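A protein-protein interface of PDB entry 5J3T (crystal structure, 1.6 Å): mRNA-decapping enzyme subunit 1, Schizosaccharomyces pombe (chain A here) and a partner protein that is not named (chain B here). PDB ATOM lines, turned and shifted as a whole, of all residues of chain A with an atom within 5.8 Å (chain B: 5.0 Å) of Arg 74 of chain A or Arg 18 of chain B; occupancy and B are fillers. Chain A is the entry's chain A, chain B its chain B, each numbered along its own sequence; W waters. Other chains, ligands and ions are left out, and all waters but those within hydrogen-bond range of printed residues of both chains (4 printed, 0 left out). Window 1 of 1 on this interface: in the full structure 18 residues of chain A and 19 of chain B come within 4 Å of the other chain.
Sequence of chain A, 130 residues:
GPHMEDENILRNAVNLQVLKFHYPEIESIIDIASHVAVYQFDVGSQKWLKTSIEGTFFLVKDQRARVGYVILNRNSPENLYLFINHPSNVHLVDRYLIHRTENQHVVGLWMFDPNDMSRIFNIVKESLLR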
ATOM      1  N   VAL A  18     -20.469 -10.575  15.377  1.00  0.00           N
ATOM      2  CA  VAL A  18     -19.463  -9.859  14.607  1.00  0.00           C
ATOM      3  C   VAL A  18     -19.797  -8.378  14.488  1.00  0.00           C
ATOM      4  O   VAL A  18     -18.939  -7.512  14.712  1.00  0.00           O
ATOM      5  CB  VAL A  18     -19.305 -10.535  13.243  1.00  0.00           C
ATOM      6  CG1 VAL A  18     -18.521  -9.645  12.281  1.00  0.00           C
ATOM      7  CG2 VAL A  18     -18.625 -11.906  13.429  1.00  0.00           C
ATOM      8  N   HIS A  22     -18.022  -4.419  16.407  1.00  0.00           N
ATOM      9  CA  HIS A  22     -17.766  -3.105  15.799  1.00  0.00           C
ATOM     10  C   HIS A  22     -18.778  -2.023  16.181  1.00  0.00           C
ATOM     11  O   HIS A  22     -18.397  -0.846  16.315  1.00  0.00           O
ATOM     12  CB  HIS A  22     -17.728  -3.246  14.279  1.00  0.00           C
ATOM     13  CG  HIS A  22     -16.636  -4.136  13.799  1.00  0.00           C
ATOM     14  ND1 HIS A  22     -15.304  -3.821  14.022  1.00  0.00           N
ATOM     15  CD2 HIS A  22     -16.707  -5.321  13.169  1.00  0.00           C
ATOM     16  CE1 HIS A  22     -14.611  -4.827  13.502  1.00  0.00           C
ATOM     17  NE2 HIS A  22     -15.410  -5.759  13.006  1.00  0.00           N
ATOM     18  N   HIS A  35     -22.533 -10.108  -1.456  1.00  0.00           N
ATOM     19  CA  HIS A  35     -21.800  -9.339  -2.448  1.00  0.00           C
ATOM     20  C   HIS A  35     -22.457  -8.048  -2.931  1.00  0.00           C
ATOM     21  O   HIS A  35     -22.944  -7.993  -4.076  1.00  0.00           O
ATOM     22  CB  HIS A  35     -21.564 -10.222  -3.682  1.00  0.00           C
ATOM     23  CG  HIS A  35     -20.723 -11.427  -3.438  1.00  0.00           C
ATOM     24  ND1 HIS A  35     -19.427 -11.314  -2.957  1.00  0.00           N
ATOM     25  CD2 HIS A  35     -20.989 -12.729  -3.679  1.00  0.00           C
ATOM     26  CE1 HIS A  35     -18.974 -12.550  -2.868  1.00  0.00           C
ATOM     27  NE2 HIS A  35     -19.878 -13.430  -3.286  1.00  0.00           N
ATOM     28  N   GLU A  54     -17.035  -3.332  -0.710  1.00  0.00           N
ATOM     29  CA  GLU A  54     -17.775  -4.437  -1.323  1.00  0.00           C
ATOM     30  C   GLU A  54     -17.797  -5.531  -0.258  1.00  0.00           C
ATOM     31  O   GLU A  54     -16.781  -5.825   0.387  1.00  0.00           O
ATOM     32  CB  GLU A  54     -17.051  -4.928  -2.595  1.00  0.00           C
ATOM     33  CG  GLU A  54     -17.942  -5.536  -3.669  1.00  0.00           C
ATOM     34  CD  GLU A  54     -17.507  -5.314  -5.118  1.00  0.00           C
ATOM     35  OE1 GLU A  54     -17.961  -6.087  -5.996  1.00  0.00           O
ATOM     36  OE2 GLU A  54     -16.747  -4.352  -5.386  1.00  0.00           O
ATOM     37  N   GLY A  55     -18.970  -6.088  -0.026  1.00  0.00           N
ATOM     38  CA  GLY A  55     -19.079  -7.169   0.934  1.00  0.00           C
ATOM     39  C   GLY A  55     -20.501  -7.521   1.276  1.00  0.00           C
ATOM     40  O   GLY A  55     -21.454  -7.128   0.578  1.00  0.00           O
ATOM     41  N   THR A  56     -20.631  -8.270   2.358  1.00  0.00           N
ATOM     42  CA  THR A  56     -21.936  -8.685   2.804  1.00  0.00           C
ATOM     43  C   THR A  56     -22.700  -7.469   3.301  1.00  0.00           C
ATOM     44  O   THR A  56     -22.196  -6.676   4.090  1.00  0.00           O
ATOM     45  CB  THR A  56     -21.870  -9.716   3.948  1.00  0.00           C
ATOM     46  OG1 THR A  56     -20.984 -10.799   3.598  1.00  0.00           O
ATOM     47  CG2 THR A  56     -23.240 -10.284   4.225  1.00  0.00           C
ATOM     48  N   LEU A  72     -20.001  -5.085   5.351  1.00  0.00           N
ATOM     49  CA  LEU A  72     -18.823  -5.599   6.035  1.00  0.00           C
ATOM     50  C   LEU A  72     -17.808  -5.786   4.963  1.00  0.00           C
ATOM     51  O   LEU A  72     -17.902  -6.718   4.170  1.00  0.00           O
ATOM     52  CB  LEU A  72     -19.210  -6.930   6.747  1.00  0.00           C
ATOM     53  CG  LEU A  72     -18.300  -7.350   7.864  1.00  0.00           C
ATOM     54  CD1 LEU A  72     -18.260  -6.289   9.014  1.00  0.00           C
ATOM     55  CD2 LEU A  72     -18.666  -8.720   8.382  1.00  0.00           C
ATOM     56  N   ASN A  73     -16.895  -4.825   4.870  1.00  0.00           N
ATOM     57  CA  ASN A  73     -16.016  -4.670   3.720  1.00  0.00           C
ATOM     58  C   ASN A  73     -14.975  -5.774   3.576  1.00  0.00           C
ATOM     59  O   ASN A  73     -14.212  -6.017   4.492  1.00  0.00           O
ATOM     60  CB  ASN A  73     -15.333  -3.308   3.815  1.00  0.00           C
ATOM     61  CG  ASN A  73     -14.645  -2.878   2.526  1.00  0.00           C
ATOM     62  OD1 ASN A  73     -14.778  -3.509   1.466  1.00  0.00           O
ATOM     63  ND2 ASN A  73     -13.835  -1.836   2.616  1.00  0.00           N
ATOM     64  N   ARG A  74     -14.917  -6.401   2.392  1.00  0.00           N
ATOM     65  CA  ARG A  74     -13.889  -7.409   2.163  1.00  0.00           C
ATOM     66  C   ARG A  74     -12.500  -6.742   1.894  1.00  0.00           C
ATOM     67  O   ARG A  74     -11.463  -7.396   2.012  1.00  0.00           O
ATOM     68  CB  ARG A  74     -14.260  -8.209   0.907  1.00  0.00           C
ATOM     69  CG  ARG A  74     -15.208  -9.347   1.163  1.00  0.00           C
ATOM     70  CD  ARG A  74     -15.328 -10.237  -0.094  1.00  0.00           C
ATOM     71  NE  ARG A  74     -15.919 -11.522   0.287  1.00  0.00           N
ATOM     72  CZ  ARG A  74     -17.220 -11.752   0.413  1.00  0.00           C
ATOM     73  NH1 ARG A  74     -18.108 -10.811   0.083  1.00  0.00           N
ATOM     74  NH2 ARG A  74     -17.651 -12.940   0.822  1.00  0.00           N
ATOM     75  N   ASN A  75     -12.508  -5.478   1.407  1.00  0.00           N
ATOM     76  CA  ASN A  75     -11.317  -4.811   0.895  1.00  0.00           C
ATOM     77  C   ASN A  75     -10.482  -4.058   1.916  1.00  0.00           C
ATOM     78  O   ASN A  75      -9.325  -3.735   1.617  1.00  0.00           O
ATOM     79  CB  ASN A  75     -11.704  -3.901  -0.280  1.00  0.00           C
ATOM     80  CG  ASN A  75     -12.203  -4.758  -1.419  1.00  0.00           C
ATOM     81  OD1 ASN A  75     -11.662  -5.834  -1.710  1.00  0.00           O
ATOM     82  ND2 ASN A  75     -13.278  -4.345  -2.041  1.00  0.00           N
ATOM     83  N   SER A  76     -11.042  -3.748   3.061  1.00  0.00           N
ATOM     84  CA  SER A  76     -10.336  -3.067   4.145  1.00  0.00           C
ATOM     85  C   SER A  76     -11.186  -3.140   5.385  1.00  0.00           C
ATOM     86  O   SER A  76     -12.361  -3.512   5.293  1.00  0.00           O
ATOM     87  CB  SER A  76     -10.035  -1.606   3.786  1.00  0.00           C
ATOM     88  OG  SER A  76     -11.120  -0.782   4.157  1.00  0.00           O
ATOM     89  N   PRO A  77     -10.643  -2.766   6.568  1.00  0.00           N
ATOM     90  CA  PRO A  77     -11.442  -2.819   7.798  1.00  0.00           C
ATOM     91  C   PRO A  77     -12.480  -1.705   7.875  1.00  0.00           C
ATOM     92  O   PRO A  77     -13.291  -1.698   8.788  1.00  0.00           O
ATOM     93  CB  PRO A  77     -10.377  -2.618   8.896  1.00  0.00           C
ATOM     94  CG  PRO A  77      -9.097  -2.914   8.252  1.00  0.00           C
ATOM     95  CD  PRO A  77      -9.259  -2.366   6.882  1.00  0.00           C
ATOM     96  N   GLU A  78     -12.447  -0.760   6.926  1.00  0.00           N
ATOM     97  CA  GLU A  78     -13.383   0.360   6.896  1.00  0.00           C
ATOM     98  C   GLU A  78     -14.686  -0.146   6.309  1.00  0.00           C
ATOM     99  O   GLU A  78     -14.761  -0.435   5.120  1.00  0.00           O
ATOM    100  CB  GLU A  78     -12.846   1.498   6.008  1.00  0.00           C
ATOM    101  CG  GLU A  78     -11.676   2.256   6.597  1.00  0.00           C
ATOM    102  CD  GLU A  78     -11.119   3.332   5.685  1.00  0.00           C
ATOM    103  OE1 GLU A  78      -9.900   3.290   5.398  1.00  0.00           O
ATOM    104  OE2 GLU A  78     -11.900   4.208   5.246  1.00  0.00           O
ATOM    105  N   ASN A  79     -15.701  -0.294   7.151  1.00  0.00           N
ATOM    106  CA  ASN A  79     -17.014  -0.749   6.669  1.00  0.00           C
ATOM    107  C   ASN A  79     -17.901   0.470   6.362  1.00  0.00           C
ATOM    108  O   ASN A  79     -17.456   1.618   6.416  1.00  0.00           O
ATOM    109  CB  ASN A  79     -17.691  -1.560   7.774  1.00  0.00           C
ATOM    110  CG  ASN A  79     -16.826  -2.688   8.255  1.00  0.00           C
ATOM    111  OD1 ASN A  79     -16.292  -3.452   7.452  1.00  0.00           O
ATOM    112  ND2 ASN A  79     -16.539  -2.723   9.560  1.00  0.00           N
ATOM    113  N   PHE B   3      -9.548  -3.954  15.760  1.00  0.00           N
ATOM    114  CA  PHE B   3      -9.441  -5.302  16.348  1.00  0.00           C
ATOM    115  C   PHE B   3      -8.480  -5.402  17.550  1.00  0.00           C
ATOM    116  O   PHE B   3      -8.235  -6.509  18.023  1.00  0.00           O
ATOM    117  CB  PHE B   3      -8.951  -6.264  15.259  1.00  0.00           C
ATOM    118  CG  PHE B   3      -9.992  -6.484  14.188  1.00  0.00           C
ATOM    119  CD1 PHE B   3     -11.013  -7.415  14.372  1.00  0.00           C
ATOM    120  CD2 PHE B   3      -9.964  -5.748  13.002  1.00  0.00           C
ATOM    121  CE1 PHE B   3     -11.971  -7.632  13.370  1.00  0.00           C
ATOM    122  CE2 PHE B   3     -10.924  -5.976  11.990  1.00  0.00           C
ATOM    123  CZ  PHE B   3     -11.925  -6.901  12.196  1.00  0.00           C
ATOM    124  N   ASP B  13     -14.295 -15.288  13.889  1.00  0.00           N
ATOM    125  CA  ASP B  13     -15.742 -15.084  13.660  1.00  0.00           C
ATOM    126  C   ASP B  13     -15.923 -13.972  12.608  1.00  0.00           C
ATOM    127  O   ASP B  13     -16.692 -14.132  11.652  1.00  0.00           O
ATOM    128  CB  ASP B  13     -16.447 -14.618  14.926  1.00  0.00           C
ATOM    129  CG  ASP B  13     -16.636 -15.669  15.992  1.00  0.00           C
ATOM    130  OD1 ASP B  13     -16.582 -16.891  15.652  1.00  0.00           O
ATOM    131  OD2 ASP B  13     -16.889 -15.283  17.141  1.00  0.00           O
ATOM    132  N   ASP B  14     -15.212 -12.865  12.807  1.00  0.00           N
ATOM    133  CA  ASP B  14     -15.283 -11.708  11.879  1.00  0.00           C
ATOM    134  C   ASP B  14     -14.898 -12.127  10.458  1.00  0.00           C
ATOM    135  O   ASP B  14     -15.624 -11.866   9.495  1.00  0.00           O
ATOM    136  CB  ASP B  14     -14.367 -10.582  12.346  1.00  0.00           C
ATOM    137  CG  ASP B  14     -14.505  -9.315  11.504  1.00  0.00           C
ATOM    138  OD1 ASP B  14     -13.968  -9.292  10.371  1.00  0.00           O
ATOM    139  OD2 ASP B  14     -15.049  -8.318  12.019  1.00  0.00           O
ATOM    140  N   LEU B  15     -13.747 -12.816  10.326  1.00  0.00           N
ATOM    141  CA  LEU B  15     -13.299 -13.243   9.002  1.00  0.00           C
ATOM    142  C   LEU B  15     -14.300 -14.229   8.381  1.00  0.00           C
ATOM    143  O   LEU B  15     -14.516 -14.169   7.169  1.00  0.00           O
ATOM    144  CB  LEU B  15     -11.890 -13.851   9.052  1.00  0.00           C
ATOM    145  CG  LEU B  15     -10.816 -12.845   9.439  1.00  0.00           C
ATOM    146  CD1 LEU B  15      -9.501 -13.584   9.799  1.00  0.00           C
ATOM    147  CD2 LEU B  15     -10.610 -11.781   8.328  1.00  0.00           C
ATOM    148  N   SER B  16     -14.897 -15.114   9.192  1.00  0.00           N
ATOM    149  CA  SER B  16     -15.893 -16.049   8.656  1.00  0.00           C
ATOM    150  C   SER B  16     -17.080 -15.258   8.111  1.00  0.00           C
ATOM    151  O   SER B  16     -17.491 -15.471   6.971  1.00  0.00           O
ATOM    152  CB  SER B  16     -16.368 -17.020   9.737  1.00  0.00           C
ATOM    153  OG  SER B  16     -17.357 -17.882   9.196  1.00  0.00           O
ATOM    154  N   ALA B  17     -17.643 -14.333   8.911  1.00  0.00           N
ATOM    155  CA  ALA B  17     -18.780 -13.534   8.423  1.00  0.00           C
ATOM    156  C   ALA B  17     -18.422 -12.691   7.219  1.00  0.00           C
ATOM    157  O   ALA B  17     -19.231 -12.540   6.291  1.00  0.00           O
ATOM    158  CB  ALA B  17     -19.327 -12.638   9.535  1.00  0.00           C
ATOM    159  N   ARG B  18     -17.216 -12.147   7.227  1.00  0.00           N
ATOM    160  CA  ARG B  18     -16.798 -11.224   6.166  1.00  0.00           C
ATOM    161  C   ARG B  18     -16.481 -11.933   4.847  1.00  0.00           C
ATOM    162  O   ARG B  18     -16.609 -11.301   3.782  1.00  0.00           O
ATOM    163  CB  ARG B  18     -15.591 -10.439   6.686  1.00  0.00           C
ATOM    164  CG  ARG B  18     -15.150  -9.226   5.849  1.00  0.00           C
ATOM    165  CD  ARG B  18     -13.988  -8.454   6.478  1.00  0.00           C
ATOM    166  NE  ARG B  18     -14.240  -8.031   7.868  1.00  0.00           N
ATOM    167  CZ  ARG B  18     -14.462  -6.770   8.229  1.00  0.00           C
ATOM    168  NH1 ARG B  18     -14.474  -5.802   7.318  1.00  0.00           N
ATOM    169  NH2 ARG B  18     -14.673  -6.467   9.507  1.00  0.00           N
ATOM    170  N   PHE B  19     -16.036 -13.240   4.902  1.00  0.00           N
ATOM    171  CA  PHE B  19     -15.583 -13.879   3.661  1.00  0.00           C
ATOM    172  C   PHE B  19     -16.291 -15.147   3.237  1.00  0.00           C
ATOM    173  O   PHE B  19     -16.355 -15.419   2.027  1.00  0.00           O
ATOM    174  CB  PHE B  19     -14.080 -14.180   3.790  1.00  0.00           C
ATOM    175  CG  PHE B  19     -13.266 -12.904   3.693  1.00  0.00           C
ATOM    176  CD1 PHE B  19     -12.980 -12.333   2.452  1.00  0.00           C
ATOM    177  CD2 PHE B  19     -12.788 -12.279   4.842  1.00  0.00           C
ATOM    178  CE1 PHE B  19     -12.286 -11.133   2.373  1.00  0.00           C
ATOM    179  CE2 PHE B  19     -12.059 -11.094   4.766  1.00  0.00           C
ATOM    180  CZ  PHE B  19     -11.843 -10.504   3.535  1.00  0.00           C
ATOM    181  N   ILE B  20     -16.738 -15.974   4.206  1.00  0.00           N
ATOM    182  CA  ILE B  20     -17.271 -17.273   3.796  1.00  0.00           C
ATOM    183  C   ILE B  20     -18.669 -17.642   4.251  1.00  0.00           C
ATOM    184  O   ILE B  20     -19.358 -18.390   3.526  1.00  0.00           O
ATOM    185  CB  ILE B  20     -16.287 -18.424   4.176  1.00  0.00           C
ATOM    186  CG1 ILE B  20     -15.972 -18.506   5.676  1.00  0.00           C
ATOM    187  CG2 ILE B  20     -14.944 -18.372   3.338  1.00  0.00           C
ATOM    188  CD1 ILE B  20     -15.154 -19.905   6.016  1.00  0.00           C
ATOM    189  N   LEU B  23     -21.842 -16.338   1.853  1.00  0.00           N
ATOM    190  CA  LEU B  23     -21.731 -16.499   0.390  1.00  0.00           C
ATOM    191  C   LEU B  23     -22.957 -17.078  -0.254  1.00  0.00           C
ATOM    192  O   LEU B  23     -23.629 -17.870   0.393  1.00  0.00           O
ATOM    193  CB  LEU B  23     -20.572 -17.462   0.085  1.00  0.00           C
ATOM    194  CG  LEU B  23     -19.176 -16.968   0.425  1.00  0.00           C
ATOM    195  CD1 LEU B  23     -18.159 -18.091   0.224  1.00  0.00           C
ATOM    196  CD2 LEU B  23     -18.777 -15.727  -0.454  1.00  0.00           C
ATOM    197  N   GLN B  37     -11.835 -17.067  -1.424  1.00  0.00           N
ATOM    198  CA  GLN B  37     -12.266 -16.292  -0.255  1.00  0.00           C
ATOM    199  C   GLN B  37     -11.304 -16.453   0.920  1.00  0.00           C
ATOM    200  O   GLN B  37     -10.981 -15.470   1.598  1.00  0.00           O
ATOM    201  CB  GLN B  37     -13.693 -16.657   0.175  1.00  0.00           C
ATOM    202  CG  GLN B  37     -14.762 -16.240  -0.841  1.00  0.00           C
ATOM    203  CD  GLN B  37     -14.897 -14.745  -1.049  1.00  0.00           C
ATOM    204  OE1 GLN B  37     -14.304 -13.907  -0.339  1.00  0.00           O
ATOM    205  NE2 GLN B  37     -15.707 -14.382  -2.030  1.00  0.00           N
ATOM    206  N   GLN B  40      -8.211 -14.324   0.418  1.00  0.00           N
ATOM    207  CA  GLN B  40      -8.406 -12.912   0.727  1.00  0.00           C
ATOM    208  C   GLN B  40      -8.564 -12.740   2.244  1.00  0.00           C
ATOM    209  O   GLN B  40      -8.071 -11.754   2.795  1.00  0.00           O
ATOM    210  CB  GLN B  40      -9.612 -12.315   0.008  1.00  0.00           C
ATOM    211  CG  GLN B  40      -9.610 -10.798   0.128  1.00  0.00           C
ATOM    212  CD  GLN B  40     -10.630 -10.117  -0.741  1.00  0.00           C
ATOM    213  OE1 GLN B  40     -11.346 -10.749  -1.507  1.00  0.00           O
ATOM    214  NE2 GLN B  40     -10.673  -8.805  -0.675  1.00  0.00           N
ATOM    215  N   TRP B  43      -5.099 -12.711   3.745  1.00  0.00           N
ATOM    216  CA  TRP B  43      -4.504 -11.406   3.445  1.00  0.00           C
ATOM    217  C   TRP B  43      -5.035 -10.353   4.449  1.00  0.00           C
ATOM    218  O   TRP B  43      -4.253  -9.658   5.086  1.00  0.00           O
ATOM    219  CB  TRP B  43      -4.879 -10.984   2.009  1.00  0.00           C
ATOM    220  CG  TRP B  43      -4.722  -9.506   1.725  1.00  0.00           C
ATOM    221  CD1 TRP B  43      -3.554  -8.825   1.512  1.00  0.00           C
ATOM    222  CD2 TRP B  43      -5.777  -8.542   1.612  1.00  0.00           C
ATOM    223  NE1 TRP B  43      -3.813  -7.498   1.271  1.00  0.00           N
ATOM    224  CE2 TRP B  43      -5.172  -7.288   1.350  1.00  0.00           C
ATOM    225  CE3 TRP B  43      -7.171  -8.598   1.782  1.00  0.00           C
ATOM    226  CZ2 TRP B  43      -5.922  -6.118   1.200  1.00  0.00           C
ATOM    227  CZ3 TRP B  43      -7.915  -7.450   1.606  1.00  0.00           C
ATOM    228  CH2 TRP B  43      -7.294  -6.231   1.271  1.00  0.00           C
ATOM    229  N   PHE B  44      -6.373 -10.298   4.628  1.00  0.00           N
ATOM    230  CA  PHE B  44      -7.003  -9.350   5.563  1.00  0.00           C
ATOM    231  C   PHE B  44      -6.466  -9.566   6.992  1.00  0.00           C
ATOM    232  O   PHE B  44      -6.146  -8.594   7.693  1.00  0.00           O
ATOM    233  CB  PHE B  44      -8.514  -9.575   5.508  1.00  0.00           C
ATOM    234  CG  PHE B  44      -9.356  -8.472   6.076  1.00  0.00           C
ATOM    235  CD1 PHE B  44      -9.489  -8.318   7.456  1.00  0.00           C
ATOM    236  CD2 PHE B  44     -10.076  -7.615   5.236  1.00  0.00           C
ATOM    237  CE1 PHE B  44     -10.289  -7.319   7.989  1.00  0.00           C
ATOM    238  CE2 PHE B  44     -10.901  -6.629   5.786  1.00  0.00           C
ATOM    239  CZ  PHE B  44     -10.970  -6.463   7.149  1.00  0.00           C
HETATM  240  O   HOH W   1     -16.215  -8.488  14.607  1.00  0.00           O
HETATM  241  O   HOH W   2     -18.455  -9.366   3.878  1.00  0.00           O
HETATM  242  O   HOH W   3     -12.741  -8.617  -2.967  1.00  0.00           O
HETATM  243  O   HOH W   4     -13.960  -3.818  10.388  1.00  0.00           O
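OD2 of Asp 14 of chain B sits at hydrogen-bond distance from NE2 of His 22 of chain A, at 2.8 Å. The backbone carbonyl oxygen (O) of Asn 73 of chain A sits at hydrogen-bond distance from the guanidinium group (NH1) of Arg 18 of chain B, at 2.8 Å. The backbone carbonyl oxygen (O) of Phe 19 of chain B lies within hydrogen-bond range of the guanidinium group (NH2) of Arg 74 of chain A. NE of Arg 74 of chain A is in hydrogen-bond range of OE1 of Gln 37 of chain B (2.9 Å). The backbone carbonyl oxygen (O) of Arg 74 of chain A lies within hydrogen-bond range of the side-chain amide nitrogen (NE2) of Gln 40 of chain B (3.1 Å). The side-chain amide oxygen (OD1) of Asn 75 of chain A lies within hydrogen-bond range of the side-chain amide nitrogen (NE2) of Gln 40 of chain B, at 3.3 Å. The guanidinium group of Arg 18 of chain B sits at hydrogen-bond distance from the side-chain amide oxygen of Asn 79 of chain A (3.0 Å).
O of Glu 54 of chain A sits at hydrogen-bond distance from N of Arg 74 of chain A (2.8 Å). O of Thr 56 of chain A lies within hydrogen-bond range of N of Leu 72 of chain A. OD1 of Asn 73 of chain A lies within hydrogen-bond range of N of Asn 75 of chain A, at 3.0 Å. The backbone carbonyl oxygen (O) of Glu 78 of chain A lies within hydrogen-bond range of the side-chain amide nitrogen (ND2) of Asn 73 of chain A (3.0 Å). N of Glu 78 of chain A is in hydrogen-bond range of OG of Ser 76 of chain A. The backbone carbonyl oxygen (O) of Phe 19 of chain B lies close to the side-chain amide oxygen (OE1) of Gln 37 of chain B.
His 22 of chain A touches Phe 3 of chain B (CE1 to CZ, 3.6 Å). NE2 of Gln 37 of chain B touches CE1 of His 35 of chain A, at 3.8 Å. Thr 56 of chain A touches Ala 17 of chain B. Leu 72 of chain A touches Arg 18 of chain B (CD1 to NH2, 3.6 Å). Asn 73 of chain A touches Phe 44 of chain B. Arg 74 of chain A touches Arg 18 of chain B (CZ to O, 3.5 Å). Trp 43 of chain B touches Arg 74 of chain A (CZ3 to O, 3.6 Å). Trp 43 of chain B touches Asn 75 of chain A (CH2 to O, 3.2 Å). Ser 76 of chain A touches Arg 18 of chain B. CZ of Phe 44 of chain B touches CA of Pro 77 of chain A (3.7 Å).
Of chain B, only Arg 18, Phe 19, Leu 23, Gln 37, Gln 40, Trp 43 and Phe 44 come within 4 Å of Arg 74 of chain A. Arg 18 of chain B touches just these residues of chain A: His 22 (3.6 Å), Leu 72 (3.6 Å), Asn 73 (2.8 Å), Arg 74 (3.5 Å), Ser 76 (3.7 Å) and Asn 79 (3.0 Å). Of the printed residues of chain B, Ser 76 of chain A touches Arg 18 (3.7 Å) and Phe 44 (3.5 Å). Of the printed residues of chain B, Asn 75 of chain A touches Gln 40 and Trp 43. Printed residues of chain B within 4 Å of Pro 77 of chain A: Phe 44 (3.7 Å). Gly 55 of chain A touches none of the printed residues of chain B. Leu 15 of chain B touches none of the printed residues of chain A. The nearest residue of chain A that does not touch Arg 18 of chain B is Pro 77 of chain A (4.3 Å). The nearest printed residue of chain B that does not touch Ser 76 of chain A is Trp 43 of chain B (4.8 Å).
Of the 14 printed residues of chain B, 11 touch a printed residue of chain A. Printed residues of chain B that touch a printed residue of chain A: Phe 3, Asp 13, Asp 14, Ala 17, Arg 18, Phe 19, Leu 23, Gln 37, Gln 40, Trp 43 and Phe 44. Hydrophobic or aromatic side chains of chain B that line the printed part of chain A: Phe 3, Phe 19, Leu 23, Trp 43 and Phe 44. Of the 14 printed residues of chain A, 11 touch a printed residue of chain B. Hydrophobic or aromatic side chains of chain A that line the printed part of chain B: Val 18, His 22, His 35 and Leu 72. Among the printed residues, 24 pairs touch across the chains. Among the printed residues, no Asp or Glu carboxylate lies within 4 Å of a Lys or Arg side-chain nitrogen of the other chain.
Water W2 lies within hydrogen-bond range of O of Arg 18 of chain B (2.7 Å), O of Leu 72 of chain A (2.7 Å) and N of Thr 56 of chain A (2.9 Å). Water W4 lies within hydrogen-bond range of the backbone carbonyl oxygen (O) of Pro 77 of chain A, the guanidinium group (NH2) of Arg 18 of chain B and the side-chain amide nitrogen (ND2) of Asn 79 of chain A. Water W1 lies within hydrogen-bond range of the side-chain carboxylate of Asp 14 of chain B (2.8 Å), the backbone carbonyl oxygen of Val 18 of chain A (2.9 Å) and a ring nitrogen (NE2) of His 22 of chain A (3.3 Å). Water W3 bridges the side-chain amide oxygen of Gln 40 of chain B and the side-chain amide oxygen of Asn 75 of chain A.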
